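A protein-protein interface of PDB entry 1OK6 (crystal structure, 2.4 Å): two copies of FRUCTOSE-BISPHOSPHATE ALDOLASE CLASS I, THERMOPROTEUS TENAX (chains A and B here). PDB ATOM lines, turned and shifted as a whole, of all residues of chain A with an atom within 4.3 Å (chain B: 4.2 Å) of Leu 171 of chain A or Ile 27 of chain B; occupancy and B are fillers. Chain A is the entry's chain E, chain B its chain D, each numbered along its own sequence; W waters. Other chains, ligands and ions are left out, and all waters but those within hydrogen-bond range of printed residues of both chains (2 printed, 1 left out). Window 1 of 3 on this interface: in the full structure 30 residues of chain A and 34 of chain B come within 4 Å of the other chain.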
ATOM      1  N   ILE A 113      11.631 -25.328  34.406  1.00  0.00           N
ATOM      2  CA  ILE A 113      11.222 -24.121  35.124  1.00  0.00           C
ATOM      3  C   ILE A 113       9.877 -24.441  35.789  1.00  0.00           C
ATOM      4  O   ILE A 113       9.120 -25.294  35.305  1.00  0.00           O
ATOM      5  CB  ILE A 113      11.111 -22.914  34.146  1.00  0.00           C
ATOM      6  CG1 ILE A 113      10.188 -23.251  32.959  1.00  0.00           C
ATOM      7  CG2 ILE A 113      12.493 -22.500  33.659  1.00  0.00           C
ATOM      8  CD1 ILE A 113       9.795 -22.048  32.085  1.00  0.00           C
ATOM      9  N   PHE A 124      14.486 -18.347  36.163  1.00  0.00           N
ATOM     10  CA  PHE A 124      14.541 -17.462  34.986  1.00  0.00           C
ATOM     11  C   PHE A 124      15.931 -16.849  34.835  1.00  0.00           C
ATOM     12  O   PHE A 124      16.467 -16.779  33.730  1.00  0.00           O
ATOM     13  CB  PHE A 124      13.451 -16.354  35.046  1.00  0.00           C
ATOM     14  CG  PHE A 124      12.020 -16.878  34.953  1.00  0.00           C
ATOM     15  CD1 PHE A 124      11.743 -18.193  34.516  1.00  0.00           C
ATOM     16  CD2 PHE A 124      10.962 -16.081  35.339  1.00  0.00           C
ATOM     17  CE1 PHE A 124      10.425 -18.675  34.456  1.00  0.00           C
ATOM     18  CE2 PHE A 124       9.653 -16.539  35.283  1.00  0.00           C
ATOM     19  CZ  PHE A 124       9.360 -17.834  34.810  1.00  0.00           C
ATOM     20  N   LEU A 127      18.142 -19.666  33.790  1.00  0.00           N
ATOM     21  CA  LEU A 127      17.837 -19.916  32.384  1.00  0.00           C
ATOM     22  C   LEU A 127      18.509 -18.921  31.415  1.00  0.00           C
ATOM     23  O   LEU A 127      18.940 -19.302  30.304  1.00  0.00           O
ATOM     24  CB  LEU A 127      16.329 -19.991  32.142  1.00  0.00           C
ATOM     25  CG  LEU A 127      15.869 -20.601  30.811  1.00  0.00           C
ATOM     26  CD1 LEU A 127      16.522 -21.975  30.580  1.00  0.00           C
ATOM     27  CD2 LEU A 127      14.355 -20.715  30.734  1.00  0.00           C
ATOM     28  N   TYR A 163      -0.346 -21.761  29.355  1.00  0.00           N
ATOM     29  CA  TYR A 163       0.575 -20.770  29.879  1.00  0.00           C
ATOM     30  C   TYR A 163       1.983 -21.374  29.840  1.00  0.00           C
ATOM     31  O   TYR A 163       2.921 -20.736  29.366  1.00  0.00           O
ATOM     32  CB  TYR A 163       0.171 -20.383  31.309  1.00  0.00           C
ATOM     33  CG  TYR A 163       0.549 -18.990  31.761  1.00  0.00           C
ATOM     34  CD1 TYR A 163      -0.161 -18.355  32.783  1.00  0.00           C
ATOM     35  CD2 TYR A 163       1.594 -18.295  31.171  1.00  0.00           C
ATOM     36  CE1 TYR A 163       0.171 -17.066  33.217  1.00  0.00           C
ATOM     37  CE2 TYR A 163       1.939 -16.996  31.603  1.00  0.00           C
ATOM     38  CZ  TYR A 163       1.228 -16.400  32.632  1.00  0.00           C
ATOM     39  OH  TYR A 163       1.562 -15.136  33.074  1.00  0.00           O
ATOM     40  N   ILE A 167       5.123 -19.616  27.973  1.00  0.00           N
ATOM     41  CA  ILE A 167       6.285 -19.169  28.740  1.00  0.00           C
ATOM     42  C   ILE A 167       7.558 -19.759  28.162  1.00  0.00           C
ATOM     43  O   ILE A 167       8.524 -19.010  27.960  1.00  0.00           O
ATOM     44  CB  ILE A 167       6.146 -19.520  30.221  1.00  0.00           C
ATOM     45  CG1 ILE A 167       4.982 -18.737  30.824  1.00  0.00           C
ATOM     46  CG2 ILE A 167       7.425 -19.176  30.978  1.00  0.00           C
ATOM     47  CD1 ILE A 167       4.454 -19.336  32.089  1.00  0.00           C
ATOM     48  N   ALA A 168       7.560 -21.074  27.871  1.00  0.00           N
ATOM     49  CA  ALA A 168       8.733 -21.716  27.262  1.00  0.00           C
ATOM     50  C   ALA A 168       9.154 -21.026  25.961  1.00  0.00           C
ATOM     51  O   ALA A 168      10.338 -20.774  25.741  1.00  0.00           O
ATOM     52  CB  ALA A 168       8.496 -23.223  27.025  1.00  0.00           C
ATOM     53  N   LEU A 169       8.189 -20.712  25.105  1.00  0.00           N
ATOM     54  CA  LEU A 169       8.486 -19.999  23.862  1.00  0.00           C
ATOM     55  C   LEU A 169       9.130 -18.619  24.142  1.00  0.00           C
ATOM     56  O   LEU A 169      10.167 -18.241  23.545  1.00  0.00           O
ATOM     57  CB  LEU A 169       7.213 -19.867  22.995  1.00  0.00           C
ATOM     58  CG  LEU A 169       7.244 -18.870  21.833  1.00  0.00           C
ATOM     59  CD1 LEU A 169       8.193 -19.313  20.716  1.00  0.00           C
ATOM     60  CD2 LEU A 169       5.856 -18.650  21.282  1.00  0.00           C
ATOM     61  N   GLU A 170       8.506 -17.881  25.064  1.00  0.00           N
ATOM     62  CA  GLU A 170       8.935 -16.524  25.404  1.00  0.00           C
ATOM     63  C   GLU A 170      10.356 -16.537  25.935  1.00  0.00           C
ATOM     64  O   GLU A 170      11.130 -15.616  25.669  1.00  0.00           O
ATOM     65  CB  GLU A 170       8.008 -15.904  26.452  1.00  0.00           C
ATOM     66  CG  GLU A 170       6.546 -15.818  26.049  1.00  0.00           C
ATOM     67  CD  GLU A 170       6.231 -14.579  25.255  1.00  0.00           C
ATOM     68  OE1 GLU A 170       6.991 -13.589  25.359  1.00  0.00           O
ATOM     69  OE2 GLU A 170       5.222 -14.605  24.533  1.00  0.00           O
ATOM     70  N   LEU A 171      10.707 -17.581  26.686  1.00  0.00           N
ATOM     71  CA  LEU A 171      12.016 -17.604  27.355  1.00  0.00           C
ATOM     72  C   LEU A 171      13.162 -18.171  26.495  1.00  0.00           C
ATOM     73  O   LEU A 171      14.331 -18.147  26.912  1.00  0.00           O
ATOM     74  CB  LEU A 171      11.933 -18.352  28.686  1.00  0.00           C
ATOM     75  CG  LEU A 171      11.014 -17.748  29.753  1.00  0.00           C
ATOM     76  CD1 LEU A 171      10.946 -18.714  30.935  1.00  0.00           C
ATOM     77  CD2 LEU A 171      11.488 -16.359  30.197  1.00  0.00           C
ATOM     78  N   GLY A 172      12.831 -18.719  25.323  1.00  0.00           N
ATOM     79  CA  GLY A 172      13.869 -19.128  24.386  1.00  0.00           C
ATOM     80  C   GLY A 172      13.984 -20.617  24.109  1.00  0.00           C
ATOM     81  O   GLY A 172      14.920 -21.064  23.447  1.00  0.00           O
ATOM     82  N   ALA A 173      13.027 -21.394  24.590  1.00  0.00           N
ATOM     83  CA  ALA A 173      13.047 -22.824  24.355  1.00  0.00           C
ATOM     84  C   ALA A 173      13.114 -23.126  22.867  1.00  0.00           C
ATOM     85  O   ALA A 173      12.393 -22.501  22.081  1.00  0.00           O
ATOM     86  CB  ALA A 173      11.806 -23.470  24.942  1.00  0.00           C
ATOM     87  N   ASP B  24       4.745  -8.434  25.100  1.00  0.00           N
ATOM     88  CA  ASP B  24       5.368  -9.279  26.100  1.00  0.00           C
ATOM     89  C   ASP B  24       4.315 -10.018  26.904  1.00  0.00           C
ATOM     90  O   ASP B  24       4.649 -10.750  27.856  1.00  0.00           O
ATOM     91  CB  ASP B  24       6.287  -8.468  27.030  1.00  0.00           C
ATOM     92  CG  ASP B  24       5.566  -7.311  27.739  1.00  0.00           C
ATOM     93  OD1 ASP B  24       4.736  -6.612  27.098  1.00  0.00           O
ATOM     94  OD2 ASP B  24       5.793  -7.006  28.929  1.00  0.00           O
ATOM     95  N   HIS B  25       3.058  -9.829  26.522  1.00  0.00           N
ATOM     96  CA  HIS B  25       1.918 -10.413  27.232  1.00  0.00           C
ATOM     97  C   HIS B  25       1.926 -11.940  27.402  1.00  0.00           C
ATOM     98  O   HIS B  25       1.358 -12.457  28.370  1.00  0.00           O
ATOM     99  CB  HIS B  25       0.586  -9.924  26.615  1.00  0.00           C
ATOM    100  CG  HIS B  25       0.367  -8.447  26.801  1.00  0.00           C
ATOM    101  ND1 HIS B  25       1.020  -7.493  26.040  1.00  0.00           N
ATOM    102  CD2 HIS B  25      -0.391  -7.763  27.693  1.00  0.00           C
ATOM    103  CE1 HIS B  25       0.661  -6.288  26.448  1.00  0.00           C
ATOM    104  NE2 HIS B  25      -0.202  -6.425  27.440  1.00  0.00           N
ATOM    105  N   GLY B  26       2.559 -12.655  26.475  1.00  0.00           N
ATOM    106  CA  GLY B  26       2.591 -14.102  26.515  1.00  0.00           C
ATOM    107  C   GLY B  26       3.177 -14.630  27.809  1.00  0.00           C
ATOM    108  O   GLY B  26       2.729 -15.683  28.300  1.00  0.00           O
ATOM    109  N   ILE B  27       4.172 -13.927  28.360  1.00  0.00           N
ATOM    110  CA  ILE B  27       4.780 -14.345  29.614  1.00  0.00           C
ATOM    111  C   ILE B  27       4.089 -13.681  30.785  1.00  0.00           C
ATOM    112  O   ILE B  27       3.812 -14.328  31.789  1.00  0.00           O
ATOM    113  CB  ILE B  27       6.334 -14.134  29.629  1.00  0.00           C
ATOM    114  CG1 ILE B  27       6.930 -14.631  30.960  1.00  0.00           C
ATOM    115  CG2 ILE B  27       6.738 -12.655  29.348  1.00  0.00           C
ATOM    116  CD1 ILE B  27       8.440 -14.768  30.983  1.00  0.00           C
ATOM    117  N   GLU B  28       3.826 -12.380  30.653  1.00  0.00           N
ATOM    118  CA  GLU B  28       3.312 -11.565  31.758  1.00  0.00           C
ATOM    119  C   GLU B  28       1.927 -12.031  32.212  1.00  0.00           C
ATOM    120  O   GLU B  28       1.670 -12.109  33.412  1.00  0.00           O
ATOM    121  CB  GLU B  28       3.263 -10.062  31.387  1.00  0.00           C
ATOM    122  CG  GLU B  28       4.611  -9.327  31.317  1.00  0.00           C
ATOM    123  CD  GLU B  28       5.383  -9.280  32.630  1.00  0.00           C
ATOM    124  OE1 GLU B  28       4.743  -9.158  33.708  1.00  0.00           O
ATOM    125  OE2 GLU B  28       6.647  -9.378  32.586  1.00  0.00           O
ATOM    126  N   HIS B  29       1.050 -12.347  31.263  1.00  0.00           N
ATOM    127  CA  HIS B  29      -0.345 -12.647  31.573  1.00  0.00           C
ATOM    128  C   HIS B  29      -0.700 -14.048  31.086  1.00  0.00           C
ATOM    129  O   HIS B  29      -1.667 -14.652  31.552  1.00  0.00           O
ATOM    130  CB  HIS B  29      -1.307 -11.604  30.953  1.00  0.00           C
ATOM    131  CG  HIS B  29      -1.097 -10.199  31.451  1.00  0.00           C
ATOM    132  ND1 HIS B  29      -1.317  -9.829  32.764  1.00  0.00           N
ATOM    133  CD2 HIS B  29      -0.670  -9.079  30.817  1.00  0.00           C
ATOM    134  CE1 HIS B  29      -1.036  -8.546  32.918  1.00  0.00           C
ATOM    135  NE2 HIS B  29      -0.641  -8.065  31.750  1.00  0.00           N
ATOM    136  N   GLY B  30       0.081 -14.561  30.144  1.00  0.00           N
ATOM    137  CA  GLY B  30      -0.249 -15.827  29.520  1.00  0.00           C
ATOM    138  C   GLY B  30      -1.130 -15.665  28.295  1.00  0.00           C
ATOM    139  O   GLY B  30      -1.524 -14.569  27.957  1.00  0.00           O
ATOM    140  N   GLN B  61       9.779 -10.329  24.048  1.00  0.00           N
ATOM    141  CA  GLN B  61      10.717 -11.091  24.845  1.00  0.00           C
ATOM    142  C   GLN B  61      11.729 -11.767  23.900  1.00  0.00           C
ATOM    143  O   GLN B  61      11.482 -11.972  22.692  1.00  0.00           O
ATOM    144  CB  GLN B  61       9.965 -12.141  25.662  1.00  0.00           C
ATOM    145  CG  GLN B  61       9.106 -11.546  26.768  1.00  0.00           C
ATOM    146  CD  GLN B  61       9.907 -11.156  27.996  1.00  0.00           C
ATOM    147  OE1 GLN B  61      10.980 -11.719  28.255  1.00  0.00           O
ATOM    148  NE2 GLN B  61       9.390 -10.188  28.760  1.00  0.00           N
ATOM    149  N   GLY B  81      10.951 -10.569  32.624  1.00  0.00           N
ATOM    150  CA  GLY B  81       9.566 -11.009  32.587  1.00  0.00           C
ATOM    151  C   GLY B  81       9.224 -11.852  33.800  1.00  0.00           C
ATOM    152  O   GLY B  81      10.066 -12.588  34.348  1.00  0.00           O
ATOM    153  N   LYS B  82       7.967 -11.755  34.216  1.00  0.00           N
ATOM    154  CA  LYS B  82       7.430 -12.613  35.274  1.00  0.00           C
ATOM    155  C   LYS B  82       6.019 -13.034  34.878  1.00  0.00           C
ATOM    156  O   LYS B  82       5.508 -12.567  33.851  1.00  0.00           O
ATOM    157  CB  LYS B  82       7.426 -11.872  36.620  1.00  0.00           C
ATOM    158  CG  LYS B  82       6.422 -10.704  36.738  1.00  0.00           C
ATOM    159  CD  LYS B  82       6.131 -10.443  38.224  1.00  0.00           C
ATOM    160  CE  LYS B  82       4.729  -9.899  38.431  1.00  0.00           C
ATOM    161  NZ  LYS B  82       3.638 -10.938  38.385  1.00  0.00           N
ATOM    162  N   THR B  83       5.407 -13.913  35.678  1.00  0.00           N
ATOM    163  CA  THR B  83       4.078 -14.414  35.404  1.00  0.00           C
ATOM    164  C   THR B  83       3.088 -13.935  36.443  1.00  0.00           C
ATOM    165  O   THR B  83       3.481 -13.559  37.551  1.00  0.00           O
ATOM    166  CB  THR B  83       4.052 -15.962  35.376  1.00  0.00           C
ATOM    167  OG1 THR B  83       4.281 -16.473  36.702  1.00  0.00           O
ATOM    168  CG2 THR B  83       5.195 -16.526  34.537  1.00  0.00           C
ATOM    169  N   ASN B  95      15.814 -12.450  31.713  1.00  0.00           N
ATOM    170  CA  ASN B  95      16.022 -13.778  31.115  1.00  0.00           C
ATOM    171  C   ASN B  95      16.922 -13.676  29.876  1.00  0.00           C
ATOM    172  O   ASN B  95      17.115 -14.648  29.144  1.00  0.00           O
ATOM    173  CB  ASN B  95      14.675 -14.433  30.753  1.00  0.00           C
ATOM    174  CG  ASN B  95      13.807 -13.539  29.907  1.00  0.00           C
ATOM    175  OD1 ASN B  95      14.104 -13.274  28.744  1.00  0.00           O
ATOM    176  ND2 ASN B  95      12.743 -13.037  30.492  1.00  0.00           N
HETATM  177  O   HOH W   1       7.214 -11.353  23.713  1.00  0.00           O
HETATM  178  O   HOH W   2       3.721 -12.395  23.818  1.00  0.00           O
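The backbone carbonyl oxygen (O) of Ile 27 of chain B is in hydrogen-bond range of the side-chain hydroxyl (OH) of Tyr 163 of chain A (2.7 Å).
OH of Tyr 163 of chain A is in hydrogen-bond range of O of Glu 28 of chain B (3.0 Å).
N of Gly 30 of chain B lies close to OH of Tyr 163 of chain A (3.3 Å).
OH of Tyr 163 of chain A sits close to N of His 29 of chain B, at 3.4 Å.
OE1 of Gln 61 of chain B lies within hydrogen-bond range of ND2 of Asn 95 of chain B.
N of Lys 82 of chain B is in hydrogen-bond range of OE2 of Glu 28 of chain B (3.2 Å).
O of His 25 of chain B lies within hydrogen-bond range of N of Gly 30 of chain B (3.0 Å).
Among the printed residues, pairs that only touch across the chains: Phe 124 of chain A with Gly 81 of chain B (3.7 Å), Tyr 163 of chain A with Gly 26 of chain B (3.6 Å), Tyr 163 of chain A with Thr 83 of chain B (3.5 Å), Ile 167 of chain A with Thr 83 of chain B (3.8 Å), Glu 170 of chain A with Gly 26 of chain B (3.3 Å), Glu 170 of chain A with Ile 27 of chain B (3.8 Å), Glu 170 of chain A with Gln 61 of chain B (3.3 Å), Leu 171 of chain A with Ile 27 of chain B (3.5 Å) and Leu 171 of chain A with Asn 95 of chain B (3.6 Å).
Of the printed residues of chain B, Ile 167 of chain A touches Thr 83.
Of the printed residues of chain B, Leu 171 of chain A touches Ile 27 (3.5 Å) and Asn 95 (3.6 Å).
Of the printed residues of chain A, Ile 27 of chain B touches Tyr 163 (2.7 Å), Glu 170 (3.8 Å) and Leu 171 (3.5 Å).
Of the printed residues of chain A, Gly 81 of chain B touches Phe 124.
The nearest printed residue of chain B that does not touch Leu 171 of chain A is Gln 61 of chain B (5.1 Å).
The nearest printed residue of chain B that does not touch Glu 170 of chain A is Asp 24 of chain B (4.4 Å).
Hydrophobic or aromatic side chains of chain B within 4 Å of the printed part of chain A: Ile 27.
Among the printed residues, 13 pairs touch across the chains.
No position is printed for both chains.
Water W2 lies within hydrogen-bond range of the side-chain carboxylate of Glu 170 of chain A and the backbone NH of Gly 26 of chain B.
Water W1 lies within hydrogen-bond range of N of Gln 61 of chain B (2.8 Å) and OE1 of Glu 170 of chain A (2.8 Å).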
